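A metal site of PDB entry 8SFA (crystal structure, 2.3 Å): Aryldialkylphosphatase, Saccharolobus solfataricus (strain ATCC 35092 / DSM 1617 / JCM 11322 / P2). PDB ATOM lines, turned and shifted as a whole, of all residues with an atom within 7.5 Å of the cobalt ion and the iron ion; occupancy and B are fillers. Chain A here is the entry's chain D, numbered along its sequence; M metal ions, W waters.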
ATOM      1  N   HIS A  22      24.371 -28.775 -18.015  1.00  0.00           N
ATOM      2  CA  HIS A  22      24.971 -27.472 -17.679  1.00  0.00           C
ATOM      3  C   HIS A  22      26.242 -27.284 -18.509  1.00  0.00           C
ATOM      4  O   HIS A  22      27.326 -27.732 -18.109  1.00  0.00           O
ATOM      5  CB  HIS A  22      25.264 -27.391 -16.174  1.00  0.00           C
ATOM      6  CG  HIS A  22      25.653 -26.021 -15.691  1.00  0.00           C
ATOM      7  ND1 HIS A  22      25.147 -25.468 -14.533  1.00  0.00           N
ATOM      8  CD2 HIS A  22      26.508 -25.094 -16.191  1.00  0.00           C
ATOM      9  CE1 HIS A  22      25.662 -24.263 -14.346  1.00  0.00           C
ATOM     10  NE2 HIS A  22      26.494 -24.017 -15.339  1.00  0.00           N
ATOM     11  N   GLU A  23      26.102 -26.605 -19.665  1.00  0.00           N
ATOM     12  CA  GLU A  23      27.217 -26.261 -20.540  1.00  0.00           C
ATOM     13  C   GLU A  23      26.955 -24.900 -21.200  1.00  0.00           C
ATOM     14  O   GLU A  23      25.808 -24.549 -21.483  1.00  0.00           O
ATOM     15  CB  GLU A  23      27.432 -27.303 -21.656  1.00  0.00           C
ATOM     16  CG  GLU A  23      27.432 -28.759 -21.221  1.00  0.00           C
ATOM     17  CD  GLU A  23      28.695 -29.185 -20.433  1.00  0.00           C
ATOM     18  OE1 GLU A  23      28.586 -30.240 -19.771  1.00  0.00           O
ATOM     19  OE2 GLU A  23      29.760 -28.501 -20.470  1.00  0.00           O
ATOM     20  N   HIS A  24      28.042 -24.162 -21.486  1.00  0.00           N
ATOM     21  CA  HIS A  24      27.954 -22.803 -22.046  1.00  0.00           C
ATOM     22  C   HIS A  24      28.578 -22.711 -23.431  1.00  0.00           C
ATOM     23  O   HIS A  24      29.785 -22.921 -23.601  1.00  0.00           O
ATOM     24  CB  HIS A  24      28.646 -21.782 -21.132  1.00  0.00           C
ATOM     25  CG  HIS A  24      28.079 -21.720 -19.751  1.00  0.00           C
ATOM     26  ND1 HIS A  24      27.050 -20.882 -19.414  1.00  0.00           N
ATOM     27  CD2 HIS A  24      28.407 -22.398 -18.629  1.00  0.00           C
ATOM     28  CE1 HIS A  24      26.770 -21.037 -18.126  1.00  0.00           C
ATOM     29  NE2 HIS A  24      27.574 -21.950 -17.631  1.00  0.00           N
ATOM     30  N   VAL A  27      30.323 -17.089 -23.271  1.00  0.00           N
ATOM     31  CA  VAL A  27      30.154 -16.307 -22.048  1.00  0.00           C
ATOM     32  C   VAL A  27      30.926 -14.996 -22.172  1.00  0.00           C
ATOM     33  O   VAL A  27      32.124 -14.994 -22.461  1.00  0.00           O
ATOM     34  CB  VAL A  27      30.629 -17.108 -20.816  1.00  0.00           C
ATOM     35  CG1 VAL A  27      30.900 -16.197 -19.634  1.00  0.00           C
ATOM     36  CG2 VAL A  27      29.608 -18.176 -20.441  1.00  0.00           C
ATOM     37  N   ASP A  66      21.726 -24.912 -21.598  1.00  0.00           N
ATOM     38  CA  ASP A  66      22.703 -23.817 -21.573  1.00  0.00           C
ATOM     39  C   ASP A  66      22.202 -22.680 -20.680  1.00  0.00           C
ATOM     40  O   ASP A  66      21.444 -21.812 -21.145  1.00  0.00           O
ATOM     41  CB  ASP A  66      22.965 -23.320 -22.989  1.00  0.00           C
ATOM     42  CG  ASP A  66      23.985 -22.189 -23.056  1.00  0.00           C
ATOM     43  OD1 ASP A  66      24.317 -21.567 -22.029  1.00  0.00           O
ATOM     44  OD2 ASP A  66      24.478 -21.926 -24.174  1.00  0.00           O
ATOM     45  N   PRO A  67      22.646 -22.606 -19.410  1.00  0.00           N
ATOM     46  CA  PRO A  67      22.145 -21.605 -18.453  1.00  0.00           C
ATOM     47  C   PRO A  67      22.902 -20.278 -18.481  1.00  0.00           C
ATOM     48  O   PRO A  67      23.294 -19.751 -17.437  1.00  0.00           O
ATOM     49  CB  PRO A  67      22.312 -22.308 -17.113  1.00  0.00           C
ATOM     50  CG  PRO A  67      23.580 -23.150 -17.320  1.00  0.00           C
ATOM     51  CD  PRO A  67      23.576 -23.570 -18.785  1.00  0.00           C
ATOM     52  N   THR A  68      23.129 -19.737 -19.683  1.00  0.00           N
ATOM     53  CA  THR A  68      23.746 -18.431 -19.860  1.00  0.00           C
ATOM     54  C   THR A  68      22.629 -17.394 -19.870  1.00  0.00           C
ATOM     55  O   THR A  68      21.735 -17.458 -20.716  1.00  0.00           O
ATOM     56  CB  THR A  68      24.537 -18.373 -21.184  1.00  0.00           C
ATOM     57  OG1 THR A  68      25.508 -19.426 -21.243  1.00  0.00           O
ATOM     58  CG2 THR A  68      25.221 -17.031 -21.343  1.00  0.00           C
ATOM     59  N   CYS A  72      25.932 -12.747 -18.312  1.00  0.00           N
ATOM     60  CA  CYS A  72      26.916 -13.628 -18.927  1.00  0.00           C
ATOM     61  C   CYS A  72      26.822 -13.687 -20.448  1.00  0.00           C
ATOM     62  O   CYS A  72      27.465 -14.541 -21.056  1.00  0.00           O
ATOM     63  CB  CYS A  72      26.814 -15.061 -18.356  1.00  0.00           C
ATOM     64  SG  CYS A  72      27.087 -15.170 -16.560  1.00  0.00           S
ATOM     65  N   PHE A  97      22.123 -13.277 -13.337  1.00  0.00           N
ATOM     66  CA  PHE A  97      23.343 -13.853 -12.751  1.00  0.00           C
ATOM     67  C   PHE A  97      24.089 -12.724 -12.054  1.00  0.00           C
ATOM     68  O   PHE A  97      24.858 -12.005 -12.699  1.00  0.00           O
ATOM     69  CB  PHE A  97      24.234 -14.493 -13.824  1.00  0.00           C
ATOM     70  CG  PHE A  97      25.331 -15.371 -13.272  1.00  0.00           C
ATOM     71  CD1 PHE A  97      26.489 -14.808 -12.723  1.00  0.00           C
ATOM     72  CD2 PHE A  97      25.195 -16.758 -13.271  1.00  0.00           C
ATOM     73  CE1 PHE A  97      27.495 -15.614 -12.208  1.00  0.00           C
ATOM     74  CE2 PHE A  97      26.198 -17.575 -12.769  1.00  0.00           C
ATOM     75  CZ  PHE A  97      27.352 -17.003 -12.235  1.00  0.00           C
ATOM     76  N   PHE A  99      26.214 -11.655  -8.165  1.00  0.00           N
ATOM     77  CA  PHE A  99      26.760 -12.065  -6.874  1.00  0.00           C
ATOM     78  C   PHE A  99      26.504 -11.055  -5.761  1.00  0.00           C
ATOM     79  O   PHE A  99      26.546 -11.438  -4.582  1.00  0.00           O
ATOM     80  CB  PHE A  99      28.278 -12.286  -6.951  1.00  0.00           C
ATOM     81  CG  PHE A  99      28.695 -13.474  -7.778  1.00  0.00           C
ATOM     82  CD1 PHE A  99      27.777 -14.441  -8.161  1.00  0.00           C
ATOM     83  CD2 PHE A  99      30.028 -13.641  -8.154  1.00  0.00           C
ATOM     84  CE1 PHE A  99      28.170 -15.545  -8.911  1.00  0.00           C
ATOM     85  CE2 PHE A  99      30.440 -14.744  -8.915  1.00  0.00           C
ATOM     86  CZ  PHE A  99      29.512 -15.691  -9.305  1.00  0.00           C
ATOM     87  N   KCX A 137      17.448 -19.423 -14.151  1.00  0.00           N
ATOM     88  CA  KCX A 137      18.803 -19.533 -13.658  1.00  0.00           C
ATOM     89  CB  KCX A 137      19.784 -19.511 -14.824  1.00  0.00           C
ATOM     90  CG  KCX A 137      21.227 -19.392 -14.435  1.00  0.00           C
ATOM     91  CD  KCX A 137      21.666 -20.577 -13.619  1.00  0.00           C
ATOM     92  CE  KCX A 137      23.064 -20.373 -13.119  1.00  0.00           C
ATOM     93  NZ  KCX A 137      24.017 -20.260 -14.258  1.00  0.00           N
ATOM     94  C   KCX A 137      19.099 -18.394 -12.669  1.00  0.00           C
ATOM     95  O   KCX A 137      18.936 -17.244 -12.997  1.00  0.00           O
ATOM     96  CX  KCX A 137      25.238 -20.746 -14.102  1.00  0.00           C
ATOM     97  OQ1 KCX A 137      26.096 -20.713 -15.002  1.00  0.00           O
ATOM     98  OQ2 KCX A 137      25.518 -21.260 -13.027  1.00  0.00           O
ATOM     99  N   ILE A 138      19.482 -18.740 -11.450  1.00  0.00           N
ATOM    100  CA  ILE A 138      19.768 -17.730 -10.440  1.00  0.00           C
ATOM    101  C   ILE A 138      21.104 -18.064  -9.821  1.00  0.00           C
ATOM    102  O   ILE A 138      21.640 -19.168 -10.028  1.00  0.00           O
ATOM    103  CB  ILE A 138      18.651 -17.669  -9.375  1.00  0.00           C
ATOM    104  CG1 ILE A 138      18.672 -18.943  -8.540  1.00  0.00           C
ATOM    105  CG2 ILE A 138      17.264 -17.462 -10.023  1.00  0.00           C
ATOM    106  CD1 ILE A 138      17.534 -19.051  -7.580  1.00  0.00           C
ATOM    107  N   ALA A 139      21.653 -17.142  -9.020  1.00  0.00           N
ATOM    108  CA  ALA A 139      23.024 -17.335  -8.573  1.00  0.00           C
ATOM    109  C   ALA A 139      23.257 -16.696  -7.206  1.00  0.00           C
ATOM    110  O   ALA A 139      22.600 -15.718  -6.824  1.00  0.00           O
ATOM    111  CB  ALA A 139      24.041 -16.766  -9.578  1.00  0.00           C
ATOM    112  N   ASP A 141      27.115 -16.534  -4.578  1.00  0.00           N
ATOM    113  CA  ASP A 141      28.474 -17.051  -4.427  1.00  0.00           C
ATOM    114  C   ASP A 141      29.064 -16.611  -3.098  1.00  0.00           C
ATOM    115  O   ASP A 141      28.334 -16.478  -2.109  1.00  0.00           O
ATOM    116  CB  ASP A 141      29.343 -16.606  -5.606  1.00  0.00           C
ATOM    117  CG  ASP A 141      30.455 -17.608  -5.933  1.00  0.00           C
ATOM    118  OD1 ASP A 141      30.186 -18.657  -6.551  1.00  0.00           O
ATOM    119  OD2 ASP A 141      31.620 -17.356  -5.525  1.00  0.00           O
ATOM    120  N   THR A 169      20.437 -23.445 -10.330  1.00  0.00           N
ATOM    121  CA  THR A 169      21.115 -22.425  -9.544  1.00  0.00           C
ATOM    122  C   THR A 169      22.631 -22.522  -9.697  1.00  0.00           C
ATOM    123  O   THR A 169      23.189 -23.541 -10.141  1.00  0.00           O
ATOM    124  CB  THR A 169      20.769 -22.479  -8.041  1.00  0.00           C
ATOM    125  OG1 THR A 169      21.508 -23.547  -7.416  1.00  0.00           O
ATOM    126  CG2 THR A 169      19.263 -22.708  -7.825  1.00  0.00           C
ATOM    127  N   HIS A 170      23.269 -21.418  -9.367  1.00  0.00           N
ATOM    128  CA  HIS A 170      24.710 -21.322  -9.158  1.00  0.00           C
ATOM    129  C   HIS A 170      24.915 -21.058  -7.679  1.00  0.00           C
ATOM    130  O   HIS A 170      24.360 -20.091  -7.136  1.00  0.00           O
ATOM    131  CB  HIS A 170      25.311 -20.197 -10.005  1.00  0.00           C
ATOM    132  CG  HIS A 170      26.762 -19.946  -9.746  1.00  0.00           C
ATOM    133  ND1 HIS A 170      27.747 -20.238 -10.675  1.00  0.00           N
ATOM    134  CD2 HIS A 170      27.398 -19.411  -8.676  1.00  0.00           C
ATOM    135  CE1 HIS A 170      28.927 -19.898 -10.176  1.00  0.00           C
ATOM    136  NE2 HIS A 170      28.744 -19.379  -8.977  1.00  0.00           N
ATOM    137  N   SER A 171      25.692 -21.900  -7.024  1.00  0.00           N
ATOM    138  CA  SER A 171      25.998 -21.684  -5.621  1.00  0.00           C
ATOM    139  C   SER A 171      27.488 -21.937  -5.405  1.00  0.00           C
ATOM    140  O   SER A 171      28.187 -22.465  -6.272  1.00  0.00           O
ATOM    141  CB  SER A 171      25.143 -22.572  -4.717  1.00  0.00           C
ATOM    142  OG  SER A 171      25.787 -23.812  -4.565  1.00  0.00           O
ATOM    143  N   GLY A 198      23.285 -26.074  -7.925  1.00  0.00           N
ATOM    144  CA  GLY A 198      24.465 -26.253  -8.731  1.00  0.00           C
ATOM    145  C   GLY A 198      25.814 -26.116  -8.011  1.00  0.00           C
ATOM    146  O   GLY A 198      25.943 -25.447  -6.973  1.00  0.00           O
ATOM    147  N   HIS A 199      26.822 -26.762  -8.593  1.00  0.00           N
ATOM    148  CA  HIS A 199      28.229 -26.686  -8.215  1.00  0.00           C
ATOM    149  C   HIS A 199      28.523 -27.382  -6.888  1.00  0.00           C
ATOM    150  O   HIS A 199      29.556 -27.123  -6.256  1.00  0.00           O
ATOM    151  CB  HIS A 199      28.712 -25.217  -8.233  1.00  0.00           C
ATOM    152  CG  HIS A 199      28.477 -24.537  -9.557  1.00  0.00           C
ATOM    153  ND1 HIS A 199      28.487 -25.218 -10.755  1.00  0.00           N
ATOM    154  CD2 HIS A 199      28.210 -23.241  -9.861  1.00  0.00           C
ATOM    155  CE1 HIS A 199      28.254 -24.372 -11.738  1.00  0.00           C
ATOM    156  NE2 HIS A 199      28.084 -23.160 -11.228  1.00  0.00           N
ATOM    157  N   ASP A 222      28.529 -30.904 -11.442  1.00  0.00           N
ATOM    158  CA  ASP A 222      28.386 -30.309 -12.764  1.00  0.00           C
ATOM    159  C   ASP A 222      29.604 -29.504 -13.230  1.00  0.00           C
ATOM    160  O   ASP A 222      29.473 -28.687 -14.146  1.00  0.00           O
ATOM    161  CB  ASP A 222      27.133 -29.422 -12.774  1.00  0.00           C
ATOM    162  CG  ASP A 222      27.156 -28.391 -11.636  1.00  0.00           C
ATOM    163  OD1 ASP A 222      28.266 -28.057 -11.159  1.00  0.00           O
ATOM    164  OD2 ASP A 222      26.066 -27.904 -11.233  1.00  0.00           O
ATOM    165  N   ARG A 223      30.785 -29.720 -12.631  1.00  0.00           N
ATOM    166  CA  ARG A 223      31.979 -28.974 -13.051  1.00  0.00           C
ATOM    167  C   ARG A 223      33.169 -29.905 -13.306  1.00  0.00           C
ATOM    168  O   ARG A 223      34.317 -29.563 -13.018  1.00  0.00           O
ATOM    169  CB  ARG A 223      32.336 -27.899 -12.033  1.00  0.00           C
ATOM    170  CG  ARG A 223      31.679 -26.536 -12.281  1.00  0.00           C
ATOM    171  CD  ARG A 223      32.018 -25.468 -11.214  1.00  0.00           C
ATOM    172  NE  ARG A 223      31.514 -24.145 -11.601  1.00  0.00           N
ATOM    173  CZ  ARG A 223      31.571 -23.040 -10.847  1.00  0.00           C
ATOM    174  NH1 ARG A 223      31.068 -21.882 -11.299  1.00  0.00           N
ATOM    175  NH2 ARG A 223      32.110 -23.073  -9.632  1.00  0.00           N
ATOM    176  N   HIS A 255      29.819 -30.482 -17.140  1.00  0.00           N
ATOM    177  CA  HIS A 255      31.176 -29.930 -17.070  1.00  0.00           C
ATOM    178  C   HIS A 255      31.254 -28.431 -16.849  1.00  0.00           C
ATOM    179  O   HIS A 255      32.344 -27.957 -16.496  1.00  0.00           O
ATOM    180  CB  HIS A 255      31.965 -30.232 -18.361  1.00  0.00           C
ATOM    181  CG  HIS A 255      31.889 -31.658 -18.820  1.00  0.00           C
ATOM    182  ND1 HIS A 255      30.887 -32.111 -19.652  1.00  0.00           N
ATOM    183  CD2 HIS A 255      32.697 -32.709 -18.568  1.00  0.00           C
ATOM    184  CE1 HIS A 255      31.084 -33.392 -19.893  1.00  0.00           C
ATOM    185  NE2 HIS A 255      32.172 -33.782 -19.266  1.00  0.00           N
ATOM    186  N   ASP A 256      30.175 -27.667 -17.054  1.00  0.00           N
ATOM    187  CA  ASP A 256      30.215 -26.203 -17.011  1.00  0.00           C
ATOM    188  C   ASP A 256      31.218 -25.644 -18.012  1.00  0.00           C
ATOM    189  O   ASP A 256      31.833 -24.601 -17.802  1.00  0.00           O
ATOM    190  CB  ASP A 256      30.532 -25.684 -15.587  1.00  0.00           C
ATOM    191  CG  ASP A 256      30.001 -24.263 -15.315  1.00  0.00           C
ATOM    192  OD1 ASP A 256      29.228 -23.724 -16.125  1.00  0.00           O
ATOM    193  OD2 ASP A 256      30.379 -23.686 -14.257  1.00  0.00           O
ATOM    194  N   TYR A 257      31.428 -26.326 -19.130  1.00  0.00           N
ATOM    195  CA  TYR A 257      32.415 -25.855 -20.090  1.00  0.00           C
ATOM    196  C   TYR A 257      31.932 -24.617 -20.829  1.00  0.00           C
ATOM    197  O   TYR A 257      30.732 -24.416 -21.059  1.00  0.00           O
ATOM    198  CB  TYR A 257      32.766 -26.969 -21.069  1.00  0.00           C
ATOM    199  CG  TYR A 257      33.909 -26.617 -22.009  1.00  0.00           C
ATOM    200  CD1 TYR A 257      35.222 -26.551 -21.537  1.00  0.00           C
ATOM    201  CD2 TYR A 257      33.671 -26.382 -23.358  1.00  0.00           C
ATOM    202  CE1 TYR A 257      36.264 -26.240 -22.386  1.00  0.00           C
ATOM    203  CE2 TYR A 257      34.713 -26.070 -24.207  1.00  0.00           C
ATOM    204  CZ  TYR A 257      36.006 -26.005 -23.724  1.00  0.00           C
ATOM    205  OH  TYR A 257      37.039 -25.674 -24.580  1.00  0.00           O
ATOM    206  N   CYS A 258      32.886 -23.753 -21.193  1.00  0.00           N
ATOM    207  CA  CYS A 258      32.618 -22.544 -21.983  1.00  0.00           C
ATOM    208  C   CYS A 258      33.415 -22.673 -23.262  1.00  0.00           C
ATOM    209  O   CYS A 258      34.642 -22.596 -23.237  1.00  0.00           O
ATOM    210  CB  CYS A 258      33.000 -21.275 -21.227  1.00  0.00           C
ATOM    211  SG  CYS A 258      32.286 -21.101 -19.563  1.00  0.00           S
HETATM  212 CO    CO M   1      27.690 -21.378 -12.318  1.00  0.00          CO
HETATM  213 FE    FE M   2      27.651 -22.151 -15.662  1.00  0.00          FE
HETATM  214  O   HOH W   1      28.972 -21.845 -13.717  1.00  0.00           O
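ND1 of His 24 is in hydrogen-bond range of OG1 of Thr 68 (2.8 Å).
The backbone carbonyl oxygen (O) of Tyr 257 lies within hydrogen-bond range of the backbone NH (N) of His 24, at 2.7 Å.
N of His 170 sits at hydrogen-bond distance from O of Ile 138, 2.9 Å away.
The guanidinium group of Arg 223 lies close to a ring nitrogen (ND1) of His 199 (3.3 Å).
ND1 of His 199 lies within hydrogen-bond range of OD1 of Asp 222, 2.9 Å away.
The backbone carbonyl oxygen of Pro 67 sits at hydrogen-bond distance from NZ of KCX 137.
NE of Arg 223 is in salt-bridge range of OD2 of Asp 256 (2.9 Å).
The backbone NH of Asp 256 is in hydrogen-bond range of the backbone carbonyl oxygen of Asp 222.
Residues that only touch the cobalt ion: Arg 223 (3.6 Å).
Within 4 Å of the cobalt ion: KCX 137, His 170, His 199 and Arg 223.
Of the 25 residues printed, 4 come within 4 Å of the iron ion.
The nearest printed residue that does not touch the iron ion is Pro 67 (4.5 Å).
The cobalt ion is bound by water W1 (2.0 Å), ND1 of His 170 (2.0 Å), NE2 of His 199 (2.1 Å) and OQ2 of KCX 137 (2.3 Å).
The iron ion is bound by a ring nitrogen (NE2) of His 24 (2.0 Å), OQ1 of KCX 137 (2.2 Å), a ring nitrogen (NE2) of His 22 (2.2 Å), the side-chain carboxylate of Asp 256 (2.3 Å) and water W1 (2.4 Å).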
